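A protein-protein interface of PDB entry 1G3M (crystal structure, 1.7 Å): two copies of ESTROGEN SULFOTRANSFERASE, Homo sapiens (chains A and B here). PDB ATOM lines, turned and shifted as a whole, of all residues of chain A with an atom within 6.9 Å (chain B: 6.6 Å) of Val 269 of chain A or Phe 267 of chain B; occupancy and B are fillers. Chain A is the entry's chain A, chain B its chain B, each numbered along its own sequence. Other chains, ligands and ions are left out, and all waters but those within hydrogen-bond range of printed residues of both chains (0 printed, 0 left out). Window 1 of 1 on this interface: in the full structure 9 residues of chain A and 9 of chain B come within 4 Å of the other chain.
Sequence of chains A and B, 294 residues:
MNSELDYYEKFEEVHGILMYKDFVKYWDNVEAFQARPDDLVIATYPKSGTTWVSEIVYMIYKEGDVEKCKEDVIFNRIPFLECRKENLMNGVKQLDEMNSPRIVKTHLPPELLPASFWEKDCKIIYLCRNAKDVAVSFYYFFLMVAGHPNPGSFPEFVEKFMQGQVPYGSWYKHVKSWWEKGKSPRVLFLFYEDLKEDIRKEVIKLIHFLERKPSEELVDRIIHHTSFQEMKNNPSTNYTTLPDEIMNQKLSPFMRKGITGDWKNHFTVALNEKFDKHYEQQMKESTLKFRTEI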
ATOM      1  N   LYS A 264       7.493  31.667 -16.105  1.00  0.00           N
ATOM      2  CA  LYS A 264       6.753  30.406 -16.045  1.00  0.00           C
ATOM      3  C   LYS A 264       6.748  29.683 -17.386  1.00  0.00           C
ATOM      4  O   LYS A 264       6.584  28.463 -17.448  1.00  0.00           O
ATOM      5  CB  LYS A 264       5.307  30.650 -15.600  1.00  0.00           C
ATOM      6  CG  LYS A 264       5.182  31.134 -14.167  1.00  0.00           C
ATOM      7  CD  LYS A 264       3.749  31.005 -13.676  1.00  0.00           C
ATOM      8  CE  LYS A 264       3.645  31.289 -12.186  1.00  0.00           C
ATOM      9  NZ  LYS A 264       2.297  30.933 -11.654  1.00  0.00           N
ATOM     10  N   HIS A 266       9.319  29.595 -19.356  1.00  0.00           N
ATOM     11  CA  HIS A 266      10.680  29.193 -19.698  1.00  0.00           C
ATOM     12  C   HIS A 266      11.376  28.281 -18.690  1.00  0.00           C
ATOM     13  O   HIS A 266      12.097  27.365 -19.079  1.00  0.00           O
ATOM     14  CB  HIS A 266      11.531  30.438 -19.965  1.00  0.00           C
ATOM     15  CG  HIS A 266      11.052  31.246 -21.132  1.00  0.00           C
ATOM     16  ND1 HIS A 266      10.066  32.205 -21.022  1.00  0.00           N
ATOM     17  CD2 HIS A 266      11.373  31.187 -22.446  1.00  0.00           C
ATOM     18  CE1 HIS A 266       9.801  32.700 -22.219  1.00  0.00           C
ATOM     19  NE2 HIS A 266      10.579  32.099 -23.100  1.00  0.00           N
ATOM     20  N   PHE A 267      11.170  28.528 -17.403  1.00  0.00           N
ATOM     21  CA  PHE A 267      11.782  27.689 -16.379  1.00  0.00           C
ATOM     22  C   PHE A 267      11.073  26.341 -16.309  1.00  0.00           C
ATOM     23  O   PHE A 267       9.843  26.288 -16.265  1.00  0.00           O
ATOM     24  CB  PHE A 267      11.658  28.320 -14.990  1.00  0.00           C
ATOM     25  CG  PHE A 267      12.665  29.392 -14.702  1.00  0.00           C
ATOM     26  CD1 PHE A 267      12.569  30.639 -15.309  1.00  0.00           C
ATOM     27  CD2 PHE A 267      13.682  29.167 -13.783  1.00  0.00           C
ATOM     28  CE1 PHE A 267      13.474  31.654 -14.998  1.00  0.00           C
ATOM     29  CE2 PHE A 267      14.592  30.172 -13.465  1.00  0.00           C
ATOM     30  CZ  PHE A 267      14.488  31.416 -14.070  1.00  0.00           C
ATOM     31  N   THR A 268      11.835  25.254 -16.310  1.00  0.00           N
ATOM     32  CA  THR A 268      11.222  23.943 -16.156  1.00  0.00           C
ATOM     33  C   THR A 268      10.926  23.883 -14.661  1.00  0.00           C
ATOM     34  O   THR A 268      11.422  24.709 -13.889  1.00  0.00           O
ATOM     35  CB  THR A 268      12.188  22.801 -16.487  1.00  0.00           C
ATOM     36  OG1 THR A 268      13.384  22.960 -15.715  1.00  0.00           O
ATOM     37  CG2 THR A 268      12.518  22.789 -17.965  1.00  0.00           C
ATOM     38  N   VAL A 269      10.123  22.914 -14.243  1.00  0.00           N
ATOM     39  CA  VAL A 269       9.803  22.784 -12.832  1.00  0.00           C
ATOM     40  C   VAL A 269      11.088  22.552 -12.035  1.00  0.00           C
ATOM     41  O   VAL A 269      11.281  23.136 -10.973  1.00  0.00           O
ATOM     42  CB  VAL A 269       8.812  21.624 -12.605  1.00  0.00           C
ATOM     43  CG1 VAL A 269       8.633  21.360 -11.114  1.00  0.00           C
ATOM     44  CG2 VAL A 269       7.469  21.977 -13.243  1.00  0.00           C
ATOM     45  N   ALA A 270      11.978  21.726 -12.573  1.00  0.00           N
ATOM     46  CA  ALA A 270      13.239  21.430 -11.900  1.00  0.00           C
ATOM     47  C   ALA A 270      14.141  22.659 -11.793  1.00  0.00           C
ATOM     48  O   ALA A 270      14.716  22.917 -10.737  1.00  0.00           O
ATOM     49  CB  ALA A 270      13.966  20.310 -12.631  1.00  0.00           C
ATOM     50  N   LEU A 271      14.266  23.419 -12.878  1.00  0.00           N
ATOM     51  CA  LEU A 271      15.119  24.603 -12.852  1.00  0.00           C
ATOM     52  C   LEU A 271      14.565  25.631 -11.875  1.00  0.00           C
ATOM     53  O   LEU A 271      15.319  26.306 -11.171  1.00  0.00           O
ATOM     54  CB  LEU A 271      15.237  25.218 -14.252  1.00  0.00           C
ATOM     55  CG  LEU A 271      16.199  26.405 -14.380  1.00  0.00           C
ATOM     56  CD1 LEU A 271      17.613  25.952 -14.053  1.00  0.00           C
ATOM     57  CD2 LEU A 271      16.137  26.973 -15.796  1.00  0.00           C
ATOM     58  N   ASN A 272      13.243  25.738 -11.828  1.00  0.00           N
ATOM     59  CA  ASN A 272      12.583  26.683 -10.934  1.00  0.00           C
ATOM     60  C   ASN A 272      12.888  26.325  -9.479  1.00  0.00           C
ATOM     61  O   ASN A 272      13.239  27.190  -8.676  1.00  0.00           O
ATOM     62  CB  ASN A 272      11.071  26.668 -11.182  1.00  0.00           C
ATOM     63  CG  ASN A 272      10.356  27.779 -10.453  1.00  0.00           C
ATOM     64  OD1 ASN A 272      10.742  28.943 -10.555  1.00  0.00           O
ATOM     65  ND2 ASN A 272       9.309  27.433  -9.713  1.00  0.00           N
ATOM     66  N   GLU A 273      12.753  25.045  -9.145  1.00  0.00           N
ATOM     67  CA  GLU A 273      13.041  24.579  -7.796  1.00  0.00           C
ATOM     68  C   GLU A 273      14.486  24.887  -7.405  1.00  0.00           C
ATOM     69  O   GLU A 273      14.749  25.333  -6.295  1.00  0.00           O
ATOM     70  CB  GLU A 273      12.796  23.072  -7.689  1.00  0.00           C
ATOM     71  CG  GLU A 273      11.348  22.700  -7.429  1.00  0.00           C
ATOM     72  CD  GLU A 273      11.101  21.205  -7.500  1.00  0.00           C
ATOM     73  OE1 GLU A 273      12.022  20.431  -7.167  1.00  0.00           O
ATOM     74  OE2 GLU A 273       9.978  20.805  -7.879  1.00  0.00           O
ATOM     75  N   LYS A 274      15.417  24.647  -8.322  1.00  0.00           N
ATOM     76  CA  LYS A 274      16.825  24.905  -8.046  1.00  0.00           C
ATOM     77  C   LYS A 274      17.063  26.399  -7.865  1.00  0.00           C
ATOM     78  O   LYS A 274      17.750  26.827  -6.934  1.00  0.00           O
ATOM     79  CB  LYS A 274      17.698  24.386  -9.189  1.00  0.00           C
ATOM     80  CG  LYS A 274      19.189  24.578  -8.946  1.00  0.00           C
ATOM     81  CD  LYS A 274      20.030  23.883 -10.000  1.00  0.00           C
ATOM     82  CE  LYS A 274      21.514  24.006  -9.667  1.00  0.00           C
ATOM     83  NZ  LYS A 274      22.364  23.175 -10.561  1.00  0.00           N
ATOM     84  N   ALA B 131       1.242   9.964 -15.970  1.00  0.00           N
ATOM     85  CA  ALA B 131       1.081  10.623 -17.263  1.00  0.00           C
ATOM     86  C   ALA B 131       2.216  11.531 -17.719  1.00  0.00           C
ATOM     87  O   ALA B 131       2.597  11.500 -18.887  1.00  0.00           O
ATOM     88  CB  ALA B 131      -0.243  11.402 -17.283  1.00  0.00           C
ATOM     89  N   LYS B 132       2.736  12.347 -16.808  1.00  0.00           N
ATOM     90  CA  LYS B 132       3.813  13.271 -17.149  1.00  0.00           C
ATOM     91  C   LYS B 132       5.079  12.557 -17.620  1.00  0.00           C
ATOM     92  O   LYS B 132       5.686  12.963 -18.610  1.00  0.00           O
ATOM     93  CB  LYS B 132       4.131  14.174 -15.953  1.00  0.00           C
ATOM     94  CG  LYS B 132       2.950  15.017 -15.499  1.00  0.00           C
ATOM     95  CD  LYS B 132       3.333  15.879 -14.299  1.00  0.00           C
ATOM     96  CE  LYS B 132       2.137  16.580 -13.715  1.00  0.00           C
ATOM     97  NZ  LYS B 132       2.524  17.422 -12.558  1.00  0.00           N
ATOM     98  N   ASP B 133       5.480  11.502 -16.912  1.00  0.00           N
ATOM     99  CA  ASP B 133       6.673  10.751 -17.296  1.00  0.00           C
ATOM    100  C   ASP B 133       6.432   9.951 -18.564  1.00  0.00           C
ATOM    101  O   ASP B 133       7.353   9.738 -19.353  1.00  0.00           O
ATOM    102  CB  ASP B 133       7.128   9.815 -16.167  1.00  0.00           C
ATOM    103  CG  ASP B 133       7.858  10.550 -15.066  1.00  0.00           C
ATOM    104  OD1 ASP B 133       8.379  11.651 -15.341  1.00  0.00           O
ATOM    105  OD2 ASP B 133       7.927  10.022 -13.932  1.00  0.00           O
ATOM    106  N   ALA B 135       4.496  10.935 -20.979  1.00  0.00           N
ATOM    107  CA  ALA B 135       4.556  11.940 -22.041  1.00  0.00           C
ATOM    108  C   ALA B 135       5.999  12.219 -22.471  1.00  0.00           C
ATOM    109  O   ALA B 135       6.289  12.328 -23.666  1.00  0.00           O
ATOM    110  CB  ALA B 135       3.878  13.226 -21.580  1.00  0.00           C
ATOM    111  N   VAL B 136       6.903  12.316 -21.501  1.00  0.00           N
ATOM    112  CA  VAL B 136       8.307  12.572 -21.800  1.00  0.00           C
ATOM    113  C   VAL B 136       8.917  11.395 -22.547  1.00  0.00           C
ATOM    114  O   VAL B 136       9.575  11.565 -23.572  1.00  0.00           O
ATOM    115  CB  VAL B 136       9.120  12.817 -20.509  1.00  0.00           C
ATOM    116  CG1 VAL B 136      10.605  12.974 -20.842  1.00  0.00           C
ATOM    117  CG2 VAL B 136       8.605  14.060 -19.803  1.00  0.00           C
ATOM    118  N   PHE B 154       8.070  20.227 -27.264  1.00  0.00           N
ATOM    119  CA  PHE B 154       7.517  19.451 -26.164  1.00  0.00           C
ATOM    120  C   PHE B 154       6.132  19.968 -25.763  1.00  0.00           C
ATOM    121  O   PHE B 154       5.223  19.180 -25.513  1.00  0.00           O
ATOM    122  CB  PHE B 154       8.457  19.463 -24.957  1.00  0.00           C
ATOM    123  CG  PHE B 154       8.025  18.541 -23.857  1.00  0.00           C
ATOM    124  CD1 PHE B 154       7.603  19.045 -22.630  1.00  0.00           C
ATOM    125  CD2 PHE B 154       7.988  17.164 -24.067  1.00  0.00           C
ATOM    126  CE1 PHE B 154       7.148  18.189 -21.627  1.00  0.00           C
ATOM    127  CE2 PHE B 154       7.533  16.299 -23.069  1.00  0.00           C
ATOM    128  CZ  PHE B 154       7.113  16.814 -21.849  1.00  0.00           C
ATOM    129  N   VAL B 158       2.799  17.678 -25.748  1.00  0.00           N
ATOM    130  CA  VAL B 158       1.984  17.505 -24.549  1.00  0.00           C
ATOM    131  C   VAL B 158       0.524  17.850 -24.834  1.00  0.00           C
ATOM    132  O   VAL B 158      -0.385  17.245 -24.271  1.00  0.00           O
ATOM    133  CB  VAL B 158       2.521  18.359 -23.377  1.00  0.00           C
ATOM    134  CG1 VAL B 158       1.534  18.358 -22.218  1.00  0.00           C
ATOM    135  CG2 VAL B 158       3.859  17.790 -22.914  1.00  0.00           C
ATOM    136  N   ASP B 262      11.311  12.478 -14.351  1.00  0.00           N
ATOM    137  CA  ASP B 262      12.034  13.197 -15.395  1.00  0.00           C
ATOM    138  C   ASP B 262      11.143  14.302 -15.964  1.00  0.00           C
ATOM    139  O   ASP B 262      11.633  15.231 -16.611  1.00  0.00           O
ATOM    140  CB  ASP B 262      12.459  12.256 -16.527  1.00  0.00           C
ATOM    141  CG  ASP B 262      13.511  12.877 -17.435  1.00  0.00           C
ATOM    142  OD1 ASP B 262      13.534  12.552 -18.643  1.00  0.00           O
ATOM    143  OD2 ASP B 262      14.326  13.680 -16.933  1.00  0.00           O
ATOM    144  N   TRP B 263       9.837  14.217 -15.719  1.00  0.00           N
ATOM    145  CA  TRP B 263       8.935  15.244 -16.229  1.00  0.00           C
ATOM    146  C   TRP B 263       9.329  16.631 -15.727  1.00  0.00           C
ATOM    147  O   TRP B 263       9.116  17.627 -16.420  1.00  0.00           O
ATOM    148  CB  TRP B 263       7.474  14.957 -15.850  1.00  0.00           C
ATOM    149  CG  TRP B 263       7.176  15.000 -14.374  1.00  0.00           C
ATOM    150  CD1 TRP B 263       7.212  13.952 -13.501  1.00  0.00           C
ATOM    151  CD2 TRP B 263       6.784  16.147 -13.606  1.00  0.00           C
ATOM    152  NE1 TRP B 263       6.865  14.371 -12.241  1.00  0.00           N
ATOM    153  CE2 TRP B 263       6.596  15.714 -12.276  1.00  0.00           C
ATOM    154  CE3 TRP B 263       6.573  17.498 -13.917  1.00  0.00           C
ATOM    155  CZ2 TRP B 263       6.204  16.585 -11.249  1.00  0.00           C
ATOM    156  CZ3 TRP B 263       6.182  18.365 -12.895  1.00  0.00           C
ATOM    157  CH2 TRP B 263       6.002  17.902 -11.578  1.00  0.00           C
ATOM    158  N   LYS B 264       9.915  16.703 -14.533  1.00  0.00           N
ATOM    159  CA  LYS B 264      10.330  17.993 -13.979  1.00  0.00           C
ATOM    160  C   LYS B 264      11.423  18.669 -14.808  1.00  0.00           C
ATOM    161  O   LYS B 264      11.589  19.888 -14.752  1.00  0.00           O
ATOM    162  CB  LYS B 264      10.816  17.830 -12.539  1.00  0.00           C
ATOM    163  CG  LYS B 264       9.724  17.446 -11.556  1.00  0.00           C
ATOM    164  CD  LYS B 264      10.232  17.548 -10.130  1.00  0.00           C
ATOM    165  CE  LYS B 264       9.138  17.257  -9.124  1.00  0.00           C
ATOM    166  NZ  LYS B 264       9.592  17.555  -7.735  1.00  0.00           N
ATOM    167  N   ASN B 265      12.164  17.879 -15.576  1.00  0.00           N
ATOM    168  CA  ASN B 265      13.232  18.424 -16.403  1.00  0.00           C
ATOM    169  C   ASN B 265      12.731  18.846 -17.778  1.00  0.00           C
ATOM    170  O   ASN B 265      13.493  19.387 -18.586  1.00  0.00           O
ATOM    171  CB  ASN B 265      14.356  17.392 -16.559  1.00  0.00           C
ATOM    172  CG  ASN B 265      14.965  16.995 -15.233  1.00  0.00           C
ATOM    173  OD1 ASN B 265      15.358  17.852 -14.442  1.00  0.00           O
ATOM    174  ND2 ASN B 265      15.048  15.690 -14.980  1.00  0.00           N
ATOM    175  N   HIS B 266      11.450  18.616 -18.051  1.00  0.00           N
ATOM    176  CA  HIS B 266      10.907  18.966 -19.354  1.00  0.00           C
ATOM    177  C   HIS B 266       9.715  19.915 -19.346  1.00  0.00           C
ATOM    178  O   HIS B 266       9.593  20.761 -20.229  1.00  0.00           O
ATOM    179  CB  HIS B 266      10.558  17.691 -20.119  1.00  0.00           C
ATOM    180  CG  HIS B 266      11.743  16.821 -20.394  1.00  0.00           C
ATOM    181  ND1 HIS B 266      12.257  15.948 -19.460  1.00  0.00           N
ATOM    182  CD2 HIS B 266      12.548  16.732 -21.478  1.00  0.00           C
ATOM    183  CE1 HIS B 266      13.329  15.357 -19.958  1.00  0.00           C
ATOM    184  NE2 HIS B 266      13.527  15.816 -21.181  1.00  0.00           N
ATOM    185  N   PHE B 267       8.835  19.772 -18.364  1.00  0.00           N
ATOM    186  CA  PHE B 267       7.665  20.642 -18.262  1.00  0.00           C
ATOM    187  C   PHE B 267       8.020  22.005 -17.683  1.00  0.00           C
ATOM    188  O   PHE B 267       8.647  22.086 -16.627  1.00  0.00           O
ATOM    189  CB  PHE B 267       6.605  20.044 -17.328  1.00  0.00           C
ATOM    190  CG  PHE B 267       5.757  18.974 -17.947  1.00  0.00           C
ATOM    191  CD1 PHE B 267       6.281  17.713 -18.211  1.00  0.00           C
ATOM    192  CD2 PHE B 267       4.415  19.221 -18.228  1.00  0.00           C
ATOM    193  CE1 PHE B 267       5.479  16.707 -18.745  1.00  0.00           C
ATOM    194  CE2 PHE B 267       3.602  18.225 -18.762  1.00  0.00           C
ATOM    195  CZ  PHE B 267       4.132  16.965 -19.020  1.00  0.00           C
ATOM    196  N   THR B 268       7.615  23.074 -18.359  1.00  0.00           N
ATOM    197  CA  THR B 268       7.844  24.403 -17.811  1.00  0.00           C
ATOM    198  C   THR B 268       6.797  24.527 -16.706  1.00  0.00           C
ATOM    199  O   THR B 268       5.873  23.712 -16.629  1.00  0.00           O
ATOM    200  CB  THR B 268       7.593  25.518 -18.846  1.00  0.00           C
ATOM    201  OG1 THR B 268       6.261  25.399 -19.365  1.00  0.00           O
ATOM    202  CG2 THR B 268       8.604  25.432 -19.986  1.00  0.00           C
ATOM    203  N   VAL B 269       6.941  25.530 -15.849  1.00  0.00           N
ATOM    204  CA  VAL B 269       5.995  25.746 -14.765  1.00  0.00           C
ATOM    205  C   VAL B 269       4.592  25.977 -15.344  1.00  0.00           C
ATOM    206  O   VAL B 269       3.602  25.469 -14.816  1.00  0.00           O
ATOM    207  CB  VAL B 269       6.433  26.961 -13.904  1.00  0.00           C
ATOM    208  CG1 VAL B 269       5.366  27.299 -12.872  1.00  0.00           C
ATOM    209  CG2 VAL B 269       7.762  26.641 -13.204  1.00  0.00           C
ATOM    210  N   ALA B 270       4.522  26.724 -16.443  1.00  0.00           N
ATOM    211  CA  ALA B 270       3.252  27.018 -17.103  1.00  0.00           C
ATOM    212  C   ALA B 270       2.596  25.766 -17.677  1.00  0.00           C
ATOM    213  O   ALA B 270       1.410  25.518 -17.440  1.00  0.00           O
ATOM    214  CB  ALA B 270       3.460  28.041 -18.210  1.00  0.00           C
ATOM    215  N   LEU B 271       3.361  24.981 -18.432  1.00  0.00           N
ATOM    216  CA  LEU B 271       2.818  23.767 -19.030  1.00  0.00           C
ATOM    217  C   LEU B 271       2.386  22.796 -17.942  1.00  0.00           C
ATOM    218  O   LEU B 271       1.358  22.129 -18.066  1.00  0.00           O
ATOM    219  CB  LEU B 271       3.846  23.090 -19.946  1.00  0.00           C
ATOM    220  CG  LEU B 271       3.304  21.888 -20.734  1.00  0.00           C
ATOM    221  CD1 LEU B 271       2.223  22.361 -21.704  1.00  0.00           C
ATOM    222  CD2 LEU B 271       4.427  21.206 -21.501  1.00  0.00           C
ATOM    223  N   ASN B 272       3.170  22.719 -16.872  1.00  0.00           N
ATOM    224  CA  ASN B 272       2.843  21.828 -15.769  1.00  0.00           C
ATOM    225  C   ASN B 272       1.514  22.238 -15.140  1.00  0.00           C
ATOM    226  O   ASN B 272       0.675  21.388 -14.821  1.00  0.00           O
ATOM    227  CB  ASN B 272       3.949  21.859 -14.712  1.00  0.00           C
ATOM    228  CG  ASN B 272       3.733  20.827 -13.624  1.00  0.00           C
ATOM    229  OD1 ASN B 272       3.521  19.652 -13.912  1.00  0.00           O
ATOM    230  ND2 ASN B 272       3.785  21.260 -12.369  1.00  0.00           N
ATOM    231  N   GLU B 273       1.323  23.541 -14.956  1.00  0.00           N
ATOM    232  CA  GLU B 273       0.080  24.050 -14.375  1.00  0.00           C
ATOM    233  C   GLU B 273      -1.111  23.719 -15.271  1.00  0.00           C
ATOM    234  O   GLU B 273      -2.169  23.312 -14.784  1.00  0.00           O
ATOM    235  CB  GLU B 273       0.164  25.563 -14.172  1.00  0.00           C
ATOM    236  CG  GLU B 273       0.923  25.984 -12.925  1.00  0.00           C
ATOM    237  CD  GLU B 273       1.004  27.492 -12.778  1.00  0.00           C
ATOM    238  OE1 GLU B 273       0.088  28.190 -13.263  1.00  0.00           O
ATOM    239  OE2 GLU B 273       1.973  27.983 -12.165  1.00  0.00           O
ATOM    240  N   PHE B 275      -1.286  21.298 -17.544  1.00  0.00           N
ATOM    241  CA  PHE B 275      -1.455  19.853 -17.575  1.00  0.00           C
ATOM    242  C   PHE B 275      -2.185  19.350 -16.338  1.00  0.00           C
ATOM    243  O   PHE B 275      -3.096  18.523 -16.446  1.00  0.00           O
ATOM    244  CB  PHE B 275      -0.085  19.173 -17.695  1.00  0.00           C
ATOM    245  CG  PHE B 275      -0.157  17.680 -17.861  1.00  0.00           C
ATOM    246  CD1 PHE B 275      -0.349  16.849 -16.761  1.00  0.00           C
ATOM    247  CD2 PHE B 275      -0.024  17.104 -19.119  1.00  0.00           C
ATOM    248  CE1 PHE B 275      -0.405  15.468 -16.912  1.00  0.00           C
ATOM    249  CE2 PHE B 275      -0.079  15.720 -19.281  1.00  0.00           C
ATOM    250  CZ  PHE B 275      -0.269  14.903 -18.173  1.00  0.00           C
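Of the printed residues of chain B, Phe 267 of chain A touches Thr 268 and Val 269. Of chain B, only Trp 263 (3.9 Å), Lys 264 (3.4 Å), Phe 267 (2.9 Å) and Asn 272 (3.8 Å) come within 4 Å of Val 269 of chain A. Ala 135 of chain B touches none of the printed residues of chain A. Of the printed residues of chain A, Lys 264 of chain B touches Thr 268, Val 269, Ala 270 and Glu 273. Of the printed residues of chain A, Ala 270 of chain B touches Lys 264 (2.9 Å). Phe 275 of chain B touches none of the printed residues of chain A. The nearest residue of chain B that does not touch Val 269 of chain A is Thr 268 of chain B (4.1 Å). The nearest residue of chain A that does not touch Phe 267 of chain B is Phe 267 of chain A (4.4 Å).
The backbone carbonyl oxygen (O) of Phe 267 of chain A lies within hydrogen-bond range of the backbone NH (N) of Val 269 of chain B (3.0 Å). The backbone NH (N) of Ala 270 of chain A is in hydrogen-bond range of the backbone carbonyl oxygen (O) of Lys 264 of chain B, 2.9 Å away. The side-chain amino group (NZ) of Lys 264 of chain B lies within salt-bridge range of the side-chain carboxylate (OE2) of Glu 273 of chain A (3.3 Å). N of Val 269 of chain A lies within hydrogen-bond range of O of Lys 264 of chain B (3.4 Å). The backbone carbonyl oxygen (O) of Lys 264 of chain A sits at hydrogen-bond distance from the backbone NH (N) of Ala 270 of chain B (2.9 Å). The backbone carbonyl oxygen (O) of Lys 264 of chain A is in hydrogen-bond range of the backbone NH (N) of Val 269 of chain B (3.4 Å). The side-chain amino group (NZ) of Lys 264 of chain A is in salt-bridge range of the side-chain carboxylate (OE2) of Glu 273 of chain B, 3.0 Å away. The backbone NH (N) of Val 269 of chain A lies within hydrogen-bond range of the backbone carbonyl oxygen (O) of Phe 267 of chain B (2.9 Å).
Of the 10 printed residues of chain A, 7 touch a printed residue of chain B. Hydrophobic or aromatic side chains of chain A that line the printed part of chain B: Val 269 and Ala 270. Of the 20 printed residues of chain B, 9 touch a printed residue of chain A.
Thr 268 of chain B touches Lys 264 of chain A. Phe 267 of chain A touches Thr 268 of chain B. O of Lys 264 of chain B touches CB of Thr 268 of chain A, 3.4 Å away. Asn 265 of chain B touches Thr 268 of chain A (O to CG2, 3.6 Å). Phe 267 of chain B touches Thr 268 of chain A. Thr 268 of chain B touches Thr 268 of chain A. CG2 of Val 269 of chain A touches CZ3 of Trp 263 of chain B (3.9 Å). Val 269 of chain A touches Asn 272 of chain B (CG2 to CB, 3.8 Å). Asn 265 of chain B touches Ala 270 of chain A (OD1 to CB, 3.4 Å). CB of Asn 272 of chain A touches CG2 of Val 269 of chain B, at 3.9 Å.
Lys 264 of chain A touches Thr 268 of chain B, and with the chains exchanged Thr 268 of chain A touches Lys 264 of chain B. Lys 264 of chain A touches Ala 270 of chain B, and with the chains exchanged Ala 270 of chain A touches Lys 264 of chain B. Lys 264 of chain A touches Glu 273 of chain B, and with the chains exchanged Glu 273 of chain A touches Lys 264 of chain B. Phe 267 of chain A touches Val 269 of chain B, and with the chains exchanged Val 269 of chain A touches Phe 267 of chain B.
OD1 of Asp 133 of chain B sits at hydrogen-bond distance from N of Trp 263 of chain B (3.0 Å). OG1 of Thr 268 of chain A is in hydrogen-bond range of N of Leu 271 of chain A. OD2 of Asp 262 of chain B lies within hydrogen-bond range of ND2 of Asn 265 of chain B, 2.9 Å away. NZ of Lys 132 of chain B is in hydrogen-bond range of OD1 of Asn 272 of chain B, 2.8 Å away. N of Leu 271 of chain B sits at hydrogen-bond distance from OG1 of Thr 268 of chain B (3.1 Å).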
